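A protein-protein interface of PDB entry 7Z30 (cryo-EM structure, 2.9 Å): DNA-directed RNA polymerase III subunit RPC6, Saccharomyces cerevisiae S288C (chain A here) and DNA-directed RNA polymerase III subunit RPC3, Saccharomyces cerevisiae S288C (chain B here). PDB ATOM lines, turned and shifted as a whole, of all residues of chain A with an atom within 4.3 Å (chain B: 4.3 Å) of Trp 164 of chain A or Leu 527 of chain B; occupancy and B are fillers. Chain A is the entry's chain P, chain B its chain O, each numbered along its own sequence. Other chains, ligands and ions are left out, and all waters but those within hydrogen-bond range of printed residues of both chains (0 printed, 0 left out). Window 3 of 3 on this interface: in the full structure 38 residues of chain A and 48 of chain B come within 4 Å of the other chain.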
ATOM      1  N   GLY A 162      14.409   8.804  13.785  1.00  0.00           N
ATOM      2  CA  GLY A 162      13.228   8.737  12.944  1.00  0.00           C
ATOM      3  C   GLY A 162      13.496   8.137  11.577  1.00  0.00           C
ATOM      4  O   GLY A 162      14.597   7.653  11.316  1.00  0.00           O
ATOM      5  N   PRO A 163      12.487   8.167  10.701  1.00  0.00           N
ATOM      6  CA  PRO A 163      12.663   7.591   9.358  1.00  0.00           C
ATOM      7  C   PRO A 163      13.695   8.310   8.507  1.00  0.00           C
ATOM      8  O   PRO A 163      14.166   7.730   7.520  1.00  0.00           O
ATOM      9  CB  PRO A 163      11.261   7.700   8.744  1.00  0.00           C
ATOM     10  CG  PRO A 163      10.625   8.838   9.474  1.00  0.00           C
ATOM     11  CD  PRO A 163      11.151   8.759  10.879  1.00  0.00           C
ATOM     12  N   TRP A 164      14.050   9.554   8.842  1.00  0.00           N
ATOM     13  CA  TRP A 164      15.060  10.269   8.066  1.00  0.00           C
ATOM     14  C   TRP A 164      16.387   9.524   8.067  1.00  0.00           C
ATOM     15  O   TRP A 164      17.030   9.399   7.018  1.00  0.00           O
ATOM     16  CB  TRP A 164      15.244  11.683   8.615  1.00  0.00           C
ATOM     17  CG  TRP A 164      13.964  12.443   8.743  1.00  0.00           C
ATOM     18  CD1 TRP A 164      13.425  13.300   7.831  1.00  0.00           C
ATOM     19  CD2 TRP A 164      13.062  12.422   9.856  1.00  0.00           C
ATOM     20  NE1 TRP A 164      12.240  13.808   8.301  1.00  0.00           N
ATOM     21  CE2 TRP A 164      11.995  13.287   9.544  1.00  0.00           C
ATOM     22  CE3 TRP A 164      13.052  11.755  11.085  1.00  0.00           C
ATOM     23  CZ2 TRP A 164      10.930  13.502  10.415  1.00  0.00           C
ATOM     24  CZ3 TRP A 164      11.994  11.971  11.947  1.00  0.00           C
ATOM     25  CH2 TRP A 164      10.948  12.836  11.609  1.00  0.00           C
ATOM     26  N   PHE A 165      16.810   9.027   9.226  1.00  0.00           N
ATOM     27  CA  PHE A 165      17.955   8.132   9.307  1.00  0.00           C
ATOM     28  C   PHE A 165      17.577   6.792   8.689  1.00  0.00           C
ATOM     29  O   PHE A 165      16.650   6.124   9.161  1.00  0.00           O
ATOM     30  CB  PHE A 165      18.392   7.968  10.762  1.00  0.00           C
ATOM     31  CG  PHE A 165      18.957   6.611  11.086  1.00  0.00           C
ATOM     32  CD1 PHE A 165      20.211   6.237  10.634  1.00  0.00           C
ATOM     33  CD2 PHE A 165      18.233   5.714  11.855  1.00  0.00           C
ATOM     34  CE1 PHE A 165      20.730   4.992  10.937  1.00  0.00           C
ATOM     35  CE2 PHE A 165      18.744   4.468  12.161  1.00  0.00           C
ATOM     36  CZ  PHE A 165      19.995   4.106  11.702  1.00  0.00           C
ATOM     37  N   THR A 166      18.279   6.407   7.625  1.00  0.00           N
ATOM     38  CA  THR A 166      17.982   5.160   6.926  1.00  0.00           C
ATOM     39  C   THR A 166      19.229   4.697   6.190  1.00  0.00           C
ATOM     40  O   THR A 166      19.688   5.373   5.264  1.00  0.00           O
ATOM     41  CB  THR A 166      16.818   5.335   5.946  1.00  0.00           C
ATOM     42  OG1 THR A 166      15.632   5.702   6.664  1.00  0.00           O
ATOM     43  CG2 THR A 166      16.563   4.046   5.182  1.00  0.00           C
ATOM     44  N   GLU A 169      22.035   6.903   5.141  1.00  0.00           N
ATOM     45  CA  GLU A 169      21.798   7.871   4.083  1.00  0.00           C
ATOM     46  C   GLU A 169      20.524   8.645   4.385  1.00  0.00           C
ATOM     47  O   GLU A 169      19.641   8.163   5.100  1.00  0.00           O
ATOM     48  CB  GLU A 169      21.695   7.194   2.707  1.00  0.00           C
ATOM     49  CG  GLU A 169      22.997   6.568   2.219  1.00  0.00           C
ATOM     50  CD  GLU A 169      24.169   7.535   2.240  1.00  0.00           C
ATOM     51  OE1 GLU A 169      23.966   8.733   1.952  1.00  0.00           O
ATOM     52  OE2 GLU A 169      25.296   7.095   2.550  1.00  0.00           O
ATOM     53  N   LEU A 170      20.438   9.859   3.837  1.00  0.00           N
ATOM     54  CA  LEU A 170      19.343  10.768   4.150  1.00  0.00           C
ATOM     55  C   LEU A 170      18.248  10.782   3.088  1.00  0.00           C
ATOM     56  O   LEU A 170      17.576  11.808   2.928  1.00  0.00           O
ATOM     57  CB  LEU A 170      19.879  12.180   4.385  1.00  0.00           C
ATOM     58  CG  LEU A 170      20.076  12.535   5.862  1.00  0.00           C
ATOM     59  CD1 LEU A 170      21.022  13.711   6.031  1.00  0.00           C
ATOM     60  CD2 LEU A 170      18.735  12.825   6.519  1.00  0.00           C
ATOM     61  N   ASP A 171      18.066   9.685   2.348  1.00  0.00           N
ATOM     62  CA  ASP A 171      16.850   9.437   1.568  1.00  0.00           C
ATOM     63  C   ASP A 171      16.544  10.602   0.620  1.00  0.00           C
ATOM     64  O   ASP A 171      15.581  11.354   0.795  1.00  0.00           O
ATOM     65  CB  ASP A 171      15.666   9.156   2.500  1.00  0.00           C
ATOM     66  CG  ASP A 171      15.833   7.871   3.282  1.00  0.00           C
ATOM     67  OD1 ASP A 171      16.346   6.888   2.709  1.00  0.00           O
ATOM     68  OD2 ASP A 171      15.444   7.844   4.469  1.00  0.00           O
ATOM     69  N   ILE A 175      13.109  12.482   1.426  1.00  0.00           N
ATOM     70  CA  ILE A 175      12.999  13.755   2.137  1.00  0.00           C
ATOM     71  C   ILE A 175      12.620  14.881   1.184  1.00  0.00           C
ATOM     72  O   ILE A 175      11.878  15.796   1.562  1.00  0.00           O
ATOM     73  CB  ILE A 175      14.302  14.072   2.893  1.00  0.00           C
ATOM     74  CG1 ILE A 175      14.812  12.831   3.624  1.00  0.00           C
ATOM     75  CG2 ILE A 175      14.094  15.222   3.868  1.00  0.00           C
ATOM     76  CD1 ILE A 175      13.846  12.273   4.642  1.00  0.00           C
ATOM     77  N   LEU A 235       4.253  11.039  12.837  1.00  0.00           N
ATOM     78  CA  LEU A 235       5.136  12.177  13.056  1.00  0.00           C
ATOM     79  C   LEU A 235       4.880  12.771  14.433  1.00  0.00           C
ATOM     80  O   LEU A 235       3.733  13.064  14.786  1.00  0.00           O
ATOM     81  CB  LEU A 235       4.942  13.231  11.965  1.00  0.00           C
ATOM     82  CG  LEU A 235       5.466  12.801  10.594  1.00  0.00           C
ATOM     83  CD1 LEU A 235       5.187  13.858   9.545  1.00  0.00           C
ATOM     84  CD2 LEU A 235       6.955  12.492  10.663  1.00  0.00           C
ATOM     85  N   ASN A 239       8.794  16.432  15.509  1.00  0.00           N
ATOM     86  CA  ASN A 239       9.252  16.041  14.180  1.00  0.00           C
ATOM     87  C   ASN A 239       8.682  16.951  13.097  1.00  0.00           C
ATOM     88  O   ASN A 239       9.389  17.306  12.147  1.00  0.00           O
ATOM     89  CB  ASN A 239       8.896  14.580  13.905  1.00  0.00           C
ATOM     90  CG  ASN A 239       9.738  13.613  14.717  1.00  0.00           C
ATOM     91  OD1 ASN A 239       9.303  12.506  15.033  1.00  0.00           O
ATOM     92  ND2 ASN A 239      10.954  14.027  15.053  1.00  0.00           N
ATOM     93  N   LEU A 243      10.701  19.301  10.535  1.00  0.00           N
ATOM     94  CA  LEU A 243      10.457  19.387   9.097  1.00  0.00           C
ATOM     95  C   LEU A 243      10.283  20.830   8.649  1.00  0.00           C
ATOM     96  O   LEU A 243      10.893  21.262   7.664  1.00  0.00           O
ATOM     97  CB  LEU A 243       9.221  18.570   8.713  1.00  0.00           C
ATOM     98  CG  LEU A 243       9.215  17.074   9.009  1.00  0.00           C
ATOM     99  CD1 LEU A 243       8.098  16.383   8.242  1.00  0.00           C
ATOM    100  CD2 LEU A 243      10.554  16.490   8.631  1.00  0.00           C
ATOM    101  N   VAL A 246      13.420  22.654   8.659  1.00  0.00           N
ATOM    102  CA  VAL A 246      14.219  22.265   7.505  1.00  0.00           C
ATOM    103  C   VAL A 246      13.753  23.009   6.259  1.00  0.00           C
ATOM    104  O   VAL A 246      14.571  23.448   5.441  1.00  0.00           O
ATOM    105  CB  VAL A 246      14.158  20.736   7.326  1.00  0.00           C
ATOM    106  CG1 VAL A 246      14.647  20.327   5.956  1.00  0.00           C
ATOM    107  CG2 VAL A 246      14.982  20.049   8.404  1.00  0.00           C
ATOM    108  N   ASN B 523      23.758  18.997   9.844  1.00  0.00           N
ATOM    109  CA  ASN B 523      22.995  17.778   9.584  1.00  0.00           C
ATOM    110  C   ASN B 523      21.669  17.775  10.333  1.00  0.00           C
ATOM    111  O   ASN B 523      20.662  17.276   9.819  1.00  0.00           O
ATOM    112  CB  ASN B 523      23.821  16.548   9.963  1.00  0.00           C
ATOM    113  CG  ASN B 523      24.517  15.926   8.771  1.00  0.00           C
ATOM    114  OD1 ASN B 523      23.875  15.561   7.789  1.00  0.00           O
ATOM    115  ND2 ASN B 523      25.837  15.801   8.850  1.00  0.00           N
ATOM    116  N   SER B 524      21.648  18.323  11.549  1.00  0.00           N
ATOM    117  CA  SER B 524      20.418  18.303  12.335  1.00  0.00           C
ATOM    118  C   SER B 524      19.387  19.294  11.805  1.00  0.00           C
ATOM    119  O   SER B 524      18.180  19.057  11.935  1.00  0.00           O
ATOM    120  CB  SER B 524      20.728  18.593  13.803  1.00  0.00           C
ATOM    121  OG  SER B 524      21.931  17.960  14.206  1.00  0.00           O
ATOM    122  N   THR B 525      19.834  20.399  11.208  1.00  0.00           N
ATOM    123  CA  THR B 525      18.939  21.445  10.734  1.00  0.00           C
ATOM    124  C   THR B 525      18.803  21.479   9.217  1.00  0.00           C
ATOM    125  O   THR B 525      18.125  22.367   8.692  1.00  0.00           O
ATOM    126  CB  THR B 525      19.420  22.813  11.229  1.00  0.00           C
ATOM    127  OG1 THR B 525      20.729  23.077  10.706  1.00  0.00           O
ATOM    128  CG2 THR B 525      19.473  22.842  12.747  1.00  0.00           C
ATOM    129  N   ALA B 526      19.428  20.546   8.503  1.00  0.00           N
ATOM    130  CA  ALA B 526      19.374  20.522   7.046  1.00  0.00           C
ATOM    131  C   ALA B 526      18.597  19.332   6.510  1.00  0.00           C
ATOM    132  O   ALA B 526      17.647  19.517   5.745  1.00  0.00           O
ATOM    133  CB  ALA B 526      20.799  20.524   6.469  1.00  0.00           C
ATOM    134  N   LEU B 527      18.969  18.114   6.902  1.00  0.00           N
ATOM    135  CA  LEU B 527      18.272  16.884   6.529  1.00  0.00           C
ATOM    136  C   LEU B 527      18.302  16.603   5.026  1.00  0.00           C
ATOM    137  O   LEU B 527      17.445  15.873   4.519  1.00  0.00           O
ATOM    138  CB  LEU B 527      16.819  16.889   7.024  1.00  0.00           C
ATOM    139  CG  LEU B 527      16.497  16.129   8.316  1.00  0.00           C
ATOM    140  CD1 LEU B 527      17.390  16.582   9.462  1.00  0.00           C
ATOM    141  CD2 LEU B 527      15.028  16.279   8.682  1.00  0.00           C
ATOM    142  N   MET B 528      19.268  17.147   4.286  1.00  0.00           N
ATOM    143  CA  MET B 528      19.461  16.722   2.907  1.00  0.00           C
ATOM    144  C   MET B 528      20.830  16.066   2.739  1.00  0.00           C
ATOM    145  O   MET B 528      21.537  15.775   3.707  1.00  0.00           O
ATOM    146  CB  MET B 528      19.309  17.873   1.915  1.00  0.00           C
ATOM    147  CG  MET B 528      18.023  18.661   1.975  1.00  0.00           C
ATOM    148  SD  MET B 528      18.266  20.133   2.958  1.00  0.00           S
ATOM    149  CE  MET B 528      18.800  21.237   1.668  1.00  0.00           C
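CD1 of Trp 164 of chain A touches CD2 of Leu 527 of chain B, at 3.5 Å.
CD1 of Leu 170 of chain A touches OD1 of Asn 523 of chain B, at 3.8 Å.
Leu 170 of chain A touches Leu 527 of chain B (CD2 to O, 3.9 Å).
CD1 of Leu 170 of chain A touches O of Met 528 of chain B, at 3.2 Å.
Ile 175 of chain A touches Leu 527 of chain B.
Val 246 of chain A touches Thr 525 of chain B.
O of Ala 526 of chain B touches CG1 of Val 246 of chain A, 3.1 Å away.
Val 246 of chain A touches Leu 527 of chain B (CG2 to CD2, 3.8 Å).
Of chain B, only Leu 527 comes within 4 Å of Trp 164 of chain A.
Leu 527 of chain B touches just these residues of chain A: Trp 164, Leu 170, Ile 175 and Val 246.
Of the printed residues of chain B, Leu 170 of chain A touches Asn 523, Leu 527 and Met 528.
Printed residues of chain A within 4 Å of Thr 525 of chain B: Val 246.
Of the printed residues of chain A, Ala 526 of chain B touches Val 246.
Of the printed residues of chain B, Ile 175 of chain A touches Leu 527 (3.5 Å).
Of the printed residues of chain A, Met 528 of chain B touches Leu 170 (3.2 Å).
Leu 235 of chain A touches none of the printed residues of chain B.
Leu 243 of chain A touches none of the printed residues of chain B.
The nearest printed residue of chain B that does not touch Trp 164 of chain A is Ala 526 of chain B (7.8 Å).
The nearest printed residue of chain B that does not touch Val 246 of chain A is Met 528 of chain B (4.7 Å).
Of the 6 printed residues of chain B, 5 touch a printed residue of chain A.
Hydrophobic or aromatic side chains of chain B within 4 Å of the printed part of chain A: Leu 527.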
